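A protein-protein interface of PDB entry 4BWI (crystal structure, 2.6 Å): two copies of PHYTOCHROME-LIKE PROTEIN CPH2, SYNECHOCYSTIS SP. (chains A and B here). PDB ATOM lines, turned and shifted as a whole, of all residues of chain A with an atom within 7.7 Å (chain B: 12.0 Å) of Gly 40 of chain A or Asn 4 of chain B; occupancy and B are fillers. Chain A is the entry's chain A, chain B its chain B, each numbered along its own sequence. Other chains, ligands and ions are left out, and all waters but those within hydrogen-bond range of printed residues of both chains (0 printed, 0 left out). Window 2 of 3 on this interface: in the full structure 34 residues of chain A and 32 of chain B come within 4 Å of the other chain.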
ATOM      1  N   GLU A  34      -1.536  23.321 -18.321  1.00  0.00           N
ATOM      2  CA  GLU A  34      -0.901  22.131 -17.765  1.00  0.00           C
ATOM      3  C   GLU A  34       0.578  22.375 -17.495  1.00  0.00           C
ATOM      4  O   GLU A  34       1.125  21.895 -16.501  1.00  0.00           O
ATOM      5  CB  GLU A  34      -1.084  20.930 -18.695  1.00  0.00           C
ATOM      6  CG  GLU A  34      -2.512  20.409 -18.775  1.00  0.00           C
ATOM      7  CD  GLU A  34      -2.927  19.629 -17.539  1.00  0.00           C
ATOM      8  OE1 GLU A  34      -2.049  19.315 -16.705  1.00  0.00           O
ATOM      9  OE2 GLU A  34      -4.130  19.321 -17.405  1.00  0.00           O
ATOM     10  N   ALA A  35       1.221  23.128 -18.382  1.00  0.00           N
ATOM     11  CA  ALA A  35       2.627  23.475 -18.209  1.00  0.00           C
ATOM     12  C   ALA A  35       2.845  24.398 -17.006  1.00  0.00           C
ATOM     13  O   ALA A  35       3.810  24.235 -16.259  1.00  0.00           O
ATOM     14  CB  ALA A  35       3.171  24.120 -19.474  1.00  0.00           C
ATOM     15  N   ARG A  36       1.947  25.362 -16.822  1.00  0.00           N
ATOM     16  CA  ARG A  36       2.077  26.328 -15.737  1.00  0.00           C
ATOM     17  C   ARG A  36       1.879  25.671 -14.371  1.00  0.00           C
ATOM     18  O   ARG A  36       2.609  25.963 -13.423  1.00  0.00           O
ATOM     19  CB  ARG A  36       1.091  27.487 -15.911  1.00  0.00           C
ATOM     20  CG  ARG A  36       1.437  28.715 -15.074  1.00  0.00           C
ATOM     21  CD  ARG A  36       0.226  29.608 -14.844  1.00  0.00           C
ATOM     22  NE  ARG A  36      -0.782  28.944 -14.023  1.00  0.00           N
ATOM     23  CZ  ARG A  36      -0.738  28.878 -12.696  1.00  0.00           C
ATOM     24  NH1 ARG A  36       0.266  29.439 -12.036  1.00  0.00           N
ATOM     25  NH2 ARG A  36      -1.697  28.249 -12.027  1.00  0.00           N
ATOM     26  N   ILE A  37       0.891  24.786 -14.275  1.00  0.00           N
ATOM     27  CA  ILE A  37       0.637  24.060 -13.033  1.00  0.00           C
ATOM     28  C   ILE A  37       1.794  23.120 -12.698  1.00  0.00           C
ATOM     29  O   ILE A  37       2.262  23.078 -11.561  1.00  0.00           O
ATOM     30  CB  ILE A  37      -0.674  23.249 -13.107  1.00  0.00           C
ATOM     31  CG1 ILE A  37      -1.884  24.185 -13.140  1.00  0.00           C
ATOM     32  CG2 ILE A  37      -0.788  22.294 -11.932  1.00  0.00           C
ATOM     33  CD1 ILE A  37      -3.213  23.452 -13.183  1.00  0.00           C
ATOM     34  N   PHE A  38       2.256  22.374 -13.698  1.00  0.00           N
ATOM     35  CA  PHE A  38       3.343  21.418 -13.508  1.00  0.00           C
ATOM     36  C   PHE A  38       4.662  22.101 -13.153  1.00  0.00           C
ATOM     37  O   PHE A  38       5.484  21.541 -12.429  1.00  0.00           O
ATOM     38  CB  PHE A  38       3.521  20.548 -14.756  1.00  0.00           C
ATOM     39  CG  PHE A  38       4.765  19.708 -14.736  1.00  0.00           C
ATOM     40  CD1 PHE A  38       4.824  18.553 -13.976  1.00  0.00           C
ATOM     41  CD2 PHE A  38       5.877  20.075 -15.476  1.00  0.00           C
ATOM     42  CE1 PHE A  38       5.969  17.780 -13.952  1.00  0.00           C
ATOM     43  CE2 PHE A  38       7.024  19.308 -15.457  1.00  0.00           C
ATOM     44  CZ  PHE A  38       7.071  18.160 -14.694  1.00  0.00           C
ATOM     45  N   LEU A  39       4.863  23.307 -13.674  1.00  0.00           N
ATOM     46  CA  LEU A  39       6.084  24.061 -13.404  1.00  0.00           C
ATOM     47  C   LEU A  39       5.952  24.950 -12.173  1.00  0.00           C
ATOM     48  O   LEU A  39       6.945  25.265 -11.520  1.00  0.00           O
ATOM     49  CB  LEU A  39       6.479  24.904 -14.616  1.00  0.00           C
ATOM     50  CG  LEU A  39       7.000  24.142 -15.834  1.00  0.00           C
ATOM     51  CD1 LEU A  39       7.241  25.100 -16.991  1.00  0.00           C
ATOM     52  CD2 LEU A  39       8.272  23.392 -15.484  1.00  0.00           C
ATOM     53  N   GLY A  40       4.725  25.351 -11.860  1.00  0.00           N
ATOM     54  CA  GLY A  40       4.481  26.241 -10.739  1.00  0.00           C
ATOM     55  C   GLY A  40       5.091  27.615 -10.963  1.00  0.00           C
ATOM     56  O   GLY A  40       5.682  28.198 -10.053  1.00  0.00           O
ATOM     57  N   VAL A  41       4.949  28.125 -12.183  1.00  0.00           N
ATOM     58  CA  VAL A  41       5.484  29.431 -12.544  1.00  0.00           C
ATOM     59  C   VAL A  41       4.369  30.459 -12.709  1.00  0.00           C
ATOM     60  O   VAL A  41       3.188  30.128 -12.617  1.00  0.00           O
ATOM     61  CB  VAL A  41       6.307  29.366 -13.848  1.00  0.00           C
ATOM     62  CG1 VAL A  41       7.644  28.679 -13.601  1.00  0.00           C
ATOM     63  CG2 VAL A  41       5.519  28.653 -14.940  1.00  0.00           C
ATOM     64  N   ASP A  42       4.753  31.705 -12.961  1.00  0.00           N
ATOM     65  CA  ASP A  42       3.786  32.795 -13.053  1.00  0.00           C
ATOM     66  C   ASP A  42       3.013  32.806 -14.373  1.00  0.00           C
ATOM     67  O   ASP A  42       1.800  33.013 -14.380  1.00  0.00           O
ATOM     68  CB  ASP A  42       4.473  34.147 -12.832  1.00  0.00           C
ATOM     69  CG  ASP A  42       4.973  34.324 -11.405  1.00  0.00           C
ATOM     70  OD1 ASP A  42       4.549  33.551 -10.514  1.00  0.00           O
ATOM     71  OD2 ASP A  42       5.777  35.248 -11.167  1.00  0.00           O
ATOM     72  N   ARG A  43       3.709  32.585 -15.484  1.00  0.00           N
ATOM     73  CA  ARG A  43       3.072  32.687 -16.793  1.00  0.00           C
ATOM     74  C   ARG A  43       3.648  31.735 -17.844  1.00  0.00           C
ATOM     75  O   ARG A  43       4.864  31.603 -17.985  1.00  0.00           O
ATOM     76  CB  ARG A  43       3.146  34.132 -17.296  1.00  0.00           C
ATOM     77  CG  ARG A  43       2.408  34.380 -18.601  1.00  0.00           C
ATOM     78  CD  ARG A  43       2.491  35.842 -18.993  1.00  0.00           C
ATOM     79  NE  ARG A  43       3.868  36.250 -19.250  1.00  0.00           N
ATOM     80  CZ  ARG A  43       4.321  37.492 -19.104  1.00  0.00           C
ATOM     81  NH1 ARG A  43       3.508  38.456 -18.687  1.00  0.00           N
ATOM     82  NH2 ARG A  43       5.590  37.766 -19.366  1.00  0.00           N
ATOM     83  N   VAL A  44       2.760  31.071 -18.576  1.00  0.00           N
ATOM     84  CA  VAL A  44       3.159  30.275 -19.733  1.00  0.00           C
ATOM     85  C   VAL A  44       2.354  30.702 -20.954  1.00  0.00           C
ATOM     86  O   VAL A  44       1.124  30.625 -20.958  1.00  0.00           O
ATOM     87  CB  VAL A  44       2.979  28.760 -19.503  1.00  0.00           C
ATOM     88  CG1 VAL A  44       3.349  27.990 -20.763  1.00  0.00           C
ATOM     89  CG2 VAL A  44       3.827  28.294 -18.332  1.00  0.00           C
ATOM     90  N   VAL A 159       7.828  30.457 -21.211  1.00  0.00           N
ATOM     91  CA  VAL A 159       7.626  30.193 -19.794  1.00  0.00           C
ATOM     92  C   VAL A 159       8.312  31.278 -18.977  1.00  0.00           C
ATOM     93  O   VAL A 159       9.539  31.379 -18.971  1.00  0.00           O
ATOM     94  CB  VAL A 159       8.185  28.815 -19.395  1.00  0.00           C
ATOM     95  CG1 VAL A 159       8.107  28.617 -17.890  1.00  0.00           C
ATOM     96  CG2 VAL A 159       7.430  27.714 -20.121  1.00  0.00           C
ATOM     97  N   HIS A 160       7.516  32.094 -18.294  1.00  0.00           N
ATOM     98  CA  HIS A 160       8.049  33.235 -17.561  1.00  0.00           C
ATOM     99  C   HIS A 160       7.735  33.175 -16.072  1.00  0.00           C
ATOM    100  O   HIS A 160       6.650  32.753 -15.667  1.00  0.00           O
ATOM    101  CB  HIS A 160       7.523  34.547 -18.152  1.00  0.00           C
ATOM    102  CG  HIS A 160       8.095  34.879 -19.495  1.00  0.00           C
ATOM    103  ND1 HIS A 160       7.735  36.008 -20.198  1.00  0.00           N
ATOM    104  CD2 HIS A 160       9.004  34.232 -20.262  1.00  0.00           C
ATOM    105  CE1 HIS A 160       8.394  36.040 -21.343  1.00  0.00           C
ATOM    106  NE2 HIS A 160       9.170  34.974 -21.407  1.00  0.00           N
ATOM    107  N   HIS A 161       8.699  33.606 -15.264  1.00  0.00           N
ATOM    108  CA  HIS A 161       8.528  33.677 -13.818  1.00  0.00           C
ATOM    109  C   HIS A 161       9.168  34.967 -13.309  1.00  0.00           C
ATOM    110  O   HIS A 161      10.232  35.372 -13.782  1.00  0.00           O
ATOM    111  CB  HIS A 161       9.157  32.456 -13.145  1.00  0.00           C
ATOM    112  CG  HIS A 161       8.697  32.234 -11.740  1.00  0.00           C
ATOM    113  ND1 HIS A 161       7.376  32.004 -11.416  1.00  0.00           N
ATOM    114  CD2 HIS A 161       9.381  32.201 -10.570  1.00  0.00           C
ATOM    115  CE1 HIS A 161       7.267  31.843 -10.110  1.00  0.00           C
ATOM    116  NE2 HIS A 161       8.468  31.958  -9.573  1.00  0.00           N
ATOM    117  N   ARG A 165      14.586  31.273 -11.105  1.00  0.00           N
ATOM    118  CA  ARG A 165      14.062  29.915 -11.179  1.00  0.00           C
ATOM    119  C   ARG A 165      14.881  29.075 -12.150  1.00  0.00           C
ATOM    120  O   ARG A 165      14.900  29.350 -13.350  1.00  0.00           O
ATOM    121  CB  ARG A 165      12.602  29.954 -11.637  1.00  0.00           C
ATOM    122  CG  ARG A 165      11.676  28.953 -10.957  1.00  0.00           C
ATOM    123  CD  ARG A 165      11.829  27.553 -11.523  1.00  0.00           C
ATOM    124  NE  ARG A 165      10.622  26.754 -11.318  1.00  0.00           N
ATOM    125  CZ  ARG A 165      10.516  25.465 -11.626  1.00  0.00           C
ATOM    126  NH1 ARG A 165      11.549  24.816 -12.145  1.00  0.00           N
ATOM    127  NH2 ARG A 165       9.377  24.823 -11.406  1.00  0.00           N
ATOM    128  N   PHE A 167      15.542  25.412 -14.069  1.00  0.00           N
ATOM    129  CA  PHE A 167      14.728  24.294 -14.526  1.00  0.00           C
ATOM    130  C   PHE A 167      15.530  23.000 -14.570  1.00  0.00           C
ATOM    131  O   PHE A 167      16.609  22.948 -15.159  1.00  0.00           O
ATOM    132  CB  PHE A 167      14.135  24.593 -15.904  1.00  0.00           C
ATOM    133  CG  PHE A 167      13.275  25.824 -15.941  1.00  0.00           C
ATOM    134  CD1 PHE A 167      11.960  25.781 -15.507  1.00  0.00           C
ATOM    135  CD2 PHE A 167      13.782  27.025 -16.411  1.00  0.00           C
ATOM    136  CE1 PHE A 167      11.166  26.912 -15.540  1.00  0.00           C
ATOM    137  CE2 PHE A 167      12.993  28.161 -16.448  1.00  0.00           C
ATOM    138  CZ  PHE A 167      11.683  28.104 -16.012  1.00  0.00           C
ATOM    139  N   GLU A 171      12.163  18.943 -16.356  1.00  0.00           N
ATOM    140  CA  GLU A 171      11.274  19.999 -16.821  1.00  0.00           C
ATOM    141  C   GLU A 171      11.586  20.414 -18.259  1.00  0.00           C
ATOM    142  O   GLU A 171      10.683  20.769 -19.019  1.00  0.00           O
ATOM    143  CB  GLU A 171      11.328  21.197 -15.869  1.00  0.00           C
ATOM    144  CG  GLU A 171      10.739  20.888 -14.497  1.00  0.00           C
ATOM    145  CD  GLU A 171      11.145  21.890 -13.432  1.00  0.00           C
ATOM    146  OE1 GLU A 171      12.224  22.505 -13.565  1.00  0.00           O
ATOM    147  OE2 GLU A 171      10.386  22.050 -12.451  1.00  0.00           O
ATOM    148  N   ASN B   4       4.878  22.423  -9.484  1.00  0.00           N
ATOM    149  CA  ASN B   4       4.260  22.021  -8.225  1.00  0.00           C
ATOM    150  C   ASN B   4       3.599  20.646  -8.306  1.00  0.00           C
ATOM    151  O   ASN B   4       3.192  20.083  -7.288  1.00  0.00           O
ATOM    152  CB  ASN B   4       3.244  23.073  -7.768  1.00  0.00           C
ATOM    153  N   ARG B   5       3.498  20.110  -9.519  1.00  0.00           N
ATOM    154  CA  ARG B   5       2.901  18.794  -9.734  1.00  0.00           C
ATOM    155  C   ARG B   5       3.974  17.748 -10.040  1.00  0.00           C
ATOM    156  O   ARG B   5       5.001  18.060 -10.646  1.00  0.00           O
ATOM    157  CB  ARG B   5       1.879  18.853 -10.875  1.00  0.00           C
ATOM    158  CG  ARG B   5       1.184  17.529 -11.169  1.00  0.00           C
ATOM    159  CD  ARG B   5       0.311  17.619 -12.409  1.00  0.00           C
ATOM    160  NE  ARG B   5      -0.824  18.515 -12.218  1.00  0.00           N
ATOM    161  CZ  ARG B   5      -1.733  18.777 -13.152  1.00  0.00           C
ATOM    162  NH1 ARG B   5      -1.637  18.210 -14.347  1.00  0.00           N
ATOM    163  NH2 ARG B   5      -2.735  19.604 -12.893  1.00  0.00           N
ATOM    164  N   SER B   6       3.737  16.512  -9.610  1.00  0.00           N
ATOM    165  CA  SER B   6       4.650  15.412  -9.904  1.00  0.00           C
ATOM    166  C   SER B   6       4.609  15.064 -11.390  1.00  0.00           C
ATOM    167  O   SER B   6       3.672  15.433 -12.098  1.00  0.00           O
ATOM    168  CB  SER B   6       4.300  14.182  -9.065  1.00  0.00           C
ATOM    169  OG  SER B   6       2.987  13.729  -9.345  1.00  0.00           O
ATOM    170  N   LEU B   7       5.631  14.353 -11.856  1.00  0.00           N
ATOM    171  CA  LEU B   7       5.739  14.002 -13.269  1.00  0.00           C
ATOM    172  C   LEU B   7       4.766  12.894 -13.655  1.00  0.00           C
ATOM    173  O   LEU B   7       4.214  12.898 -14.756  1.00  0.00           O
ATOM    174  CB  LEU B   7       7.169  13.579 -13.610  1.00  0.00           C
ATOM    175  CG  LEU B   7       7.441  13.266 -15.083  1.00  0.00           C
ATOM    176  CD1 LEU B   7       7.250  14.510 -15.939  1.00  0.00           C
ATOM    177  CD2 LEU B   7       8.836  12.691 -15.264  1.00  0.00           C
ATOM    178  N   GLU B   8       4.564  11.948 -12.744  1.00  0.00           N
ATOM    179  CA  GLU B   8       3.680  10.812 -12.987  1.00  0.00           C
ATOM    180  C   GLU B   8       2.255  11.259 -13.297  1.00  0.00           C
ATOM    181  O   GLU B   8       1.610  10.731 -14.202  1.00  0.00           O
ATOM    182  CB  GLU B   8       3.682   9.868 -11.783  1.00  0.00           C
ATOM    183  CG  GLU B   8       2.760   8.669 -11.929  1.00  0.00           C
ATOM    184  CD  GLU B   8       2.752   7.789 -10.694  1.00  0.00           C
ATOM    185  OE1 GLU B   8       3.515   8.083  -9.750  1.00  0.00           O
ATOM    186  OE2 GLU B   8       1.983   6.805 -10.667  1.00  0.00           O
ATOM    187  N   ASP B   9       1.773  12.242 -12.542  1.00  0.00           N
ATOM    188  CA  ASP B   9       0.427  12.769 -12.735  1.00  0.00           C
ATOM    189  C   ASP B   9       0.316  13.529 -14.054  1.00  0.00           C
ATOM    190  O   ASP B   9      -0.734  13.522 -14.698  1.00  0.00           O
ATOM    191  CB  ASP B   9       0.038  13.684 -11.571  1.00  0.00           C
ATOM    192  CG  ASP B   9       0.102  12.979 -10.228  1.00  0.00           C
ATOM    193  OD1 ASP B   9      -0.046  11.739 -10.199  1.00  0.00           O
ATOM    194  OD2 ASP B   9       0.298  13.666  -9.202  1.00  0.00           O
ATOM    195  N   PHE B  10       1.404  14.178 -14.454  1.00  0.00           N
ATOM    196  CA  PHE B  10       1.407  14.989 -15.664  1.00  0.00           C
ATOM    197  C   PHE B  10       1.322  14.135 -16.925  1.00  0.00           C
ATOM    198  O   PHE B  10       0.508  14.402 -17.808  1.00  0.00           O
ATOM    199  CB  PHE B  10       2.653  15.874 -15.717  1.00  0.00           C
ATOM    200  CG  PHE B  10       2.645  16.856 -16.853  1.00  0.00           C
ATOM    201  CD1 PHE B  10       2.012  18.080 -16.720  1.00  0.00           C
ATOM    202  CD2 PHE B  10       3.263  16.553 -18.054  1.00  0.00           C
ATOM    203  CE1 PHE B  10       1.998  18.986 -17.763  1.00  0.00           C
ATOM    204  CE2 PHE B  10       3.250  17.454 -19.101  1.00  0.00           C
ATOM    205  CZ  PHE B  10       2.620  18.673 -18.954  1.00  0.00           C
ATOM    206  N   LEU B  11       2.168  13.113 -17.002  1.00  0.00           N
ATOM    207  CA  LEU B  11       2.242  12.258 -18.184  1.00  0.00           C
ATOM    208  C   LEU B  11       0.937  11.502 -18.425  1.00  0.00           C
ATOM    209  O   LEU B  11       0.556  11.256 -19.569  1.00  0.00           O
ATOM    210  CB  LEU B  11       3.403  11.272 -18.055  1.00  0.00           C
ATOM    211  CG  LEU B  11       4.781  11.889 -17.811  1.00  0.00           C
ATOM    212  CD1 LEU B  11       5.819  10.801 -17.593  1.00  0.00           C
ATOM    213  CD2 LEU B  11       5.177  12.789 -18.969  1.00  0.00           C
ATOM    214  N   ASN B  13      -1.955  12.665 -17.674  1.00  0.00           N
ATOM    215  CA  ASN B  13      -2.889  13.666 -18.176  1.00  0.00           C
ATOM    216  C   ASN B  13      -2.674  13.945 -19.659  1.00  0.00           C
ATOM    217  O   ASN B  13      -3.626  14.201 -20.397  1.00  0.00           O
ATOM    218  CB  ASN B  13      -2.783  14.966 -17.374  1.00  0.00           C
ATOM    219  CG  ASN B  13      -3.511  14.894 -16.048  1.00  0.00           C
ATOM    220  OD1 ASN B  13      -4.487  14.157 -15.902  1.00  0.00           O
ATOM    221  ND2 ASN B  13      -3.044  15.664 -15.071  1.00  0.00           N
ATOM    222  N   GLU B 202       9.946   6.936 -15.455  1.00  0.00           N
ATOM    223  CA  GLU B 202       9.515   7.547 -14.201  1.00  0.00           C
ATOM    224  C   GLU B 202       9.135   6.504 -13.153  1.00  0.00           C
ATOM    225  O   GLU B 202       9.586   6.571 -12.011  1.00  0.00           O
ATOM    226  CB  GLU B 202       8.340   8.498 -14.446  1.00  0.00           C
ATOM    227  CG  GLU B 202       7.680   9.024 -13.178  1.00  0.00           C
ATOM    228  CD  GLU B 202       8.561   9.992 -12.407  1.00  0.00           C
ATOM    229  OE1 GLU B 202       9.569  10.465 -12.973  1.00  0.00           O
ATOM    230  OE2 GLU B 202       8.241  10.283 -11.234  1.00  0.00           O
ATOM    231  N   GLN B 206      10.647   5.705  -9.132  1.00  0.00           N
ATOM    232  CA  GLN B 206       9.814   5.678  -7.933  1.00  0.00           C
ATOM    233  C   GLN B 206       9.744   4.284  -7.317  1.00  0.00           C
ATOM    234  O   GLN B 206       9.578   4.140  -6.106  1.00  0.00           O
ATOM    235  CB  GLN B 206       8.405   6.190  -8.236  1.00  0.00           C
ATOM    236  CG  GLN B 206       8.340   7.659  -8.619  1.00  0.00           C
ATOM    237  CD  GLN B 206       6.919   8.188  -8.645  1.00  0.00           C
ATOM    238  OE1 GLN B 206       5.987   7.515  -8.206  1.00  0.00           O
ATOM    239  NE2 GLN B 206       6.748   9.399  -9.162  1.00  0.00           N
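Printed residues of chain A that touch a printed residue of chain B: Glu 34, Ile 37, Phe 38, Leu 39 and Gly 40.
Among the printed residues, Asp or Glu carboxylates within 4 Å of a Lys or Arg side-chain nitrogen of the other chain: Glu 34 of chain A with Arg 5 of chain B (2.6 Å).
Glu 34 of chain A touches Phe 10 of chain B (O to CE1, 3.3 Å).
CG2 of Ile 37 of chain A touches NH2 of Arg 5 of chain B, 3.5 Å away.
Phe 38 of chain A touches Arg 5 of chain B (CD1 to O, 3.4 Å).
Ser 6 of chain B touches Phe 38 of chain A (O to CE1, 3.8 Å).
Phe 38 of chain A touches Leu 7 of chain B (CE1 to CA, 3.8 Å).
Phe 10 of chain B touches Phe 38 of chain A (CD1 to CB, 3.5 Å).
Asn 4 of chain B touches Leu 39 of chain A (N to C, 3.8 Å).
N of Gly 40 of chain A touches N of Asn 4 of chain B, 3.8 Å away.
Of chain B, only Asn 4 (3.8 Å) comes within 4 Å of Gly 40 of chain A.
No residue of chain B comes within 4 Å of Ala 35 of chain A.
No residue of chain B comes within 4 Å of Arg 36 of chain A.
Phe 38 of chain A touches just these residues of chain B: Asn 4, Arg 5, Ser 6, Leu 7 and Phe 10.
Of chain B, only Asn 4 (3.8 Å) comes within 4 Å of Leu 39 of chain A.
No residue of chain B comes within 4 Å of Val 41 of chain A.
Asp 42 of chain A touches none of the printed residues of chain B.
Of the printed residues of chain A, Phe 10 of chain B touches Glu 34 and Phe 38.
Printed residues of chain A within 4 Å of Leu 7 of chain B: Phe 38 (3.8 Å).
Printed residues of chain A within 4 Å of Arg 5 of chain B: Glu 34 (2.6 Å), Ile 37 (3.5 Å) and Phe 38 (3.4 Å).
Printed residues of chain B within 4 Å of Ile 37 of chain A: Asn 4 and Arg 5.
Gln 206 of chain B touches none of the printed residues of chain A.
The nearest residue of chain B that does not touch Gly 40 of chain A is Arg 5 of chain B (5.9 Å).
The nearest residue of chain A that does not touch Asn 4 of chain B is Arg 165 of chain A (5.4 Å).
The side-chain carboxylate (OD2) of Asp 9 of chain B lies within hydrogen-bond range of the side-chain hydroxyl (OG) of Ser 6 of chain B (2.7 Å).
The backbone carbonyl oxygen (O) of Leu 39 of chain A is in hydrogen-bond range of the guanidinium group (NH2) of Arg 165 of chain A, at 2.5 Å.
The side-chain amide nitrogen of Asn 13 of chain B lies close to the guanidinium group of Arg 5 of chain B, at 3.0 Å.
The backbone NH (N) of Asn 4 of chain B sits at hydrogen-bond distance from the backbone carbonyl oxygen (O) of Phe 38 of chain A (3.1 Å).
The backbone carbonyl oxygen (O) of Ile 37 of chain A sits at hydrogen-bond distance from the backbone NH (N) of Asn 4 of chain B (3.4 Å).
The guanidinium group (NH1) of Arg 5 of chain B lies within salt-bridge range of the side-chain carboxylate (OE1) of Glu 34 of chain A (2.6 Å).
No position is printed for both chains.
Of the 11 pairs that touch across the chains among the printed residues, none has its exchanged pair printed and touching as well.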
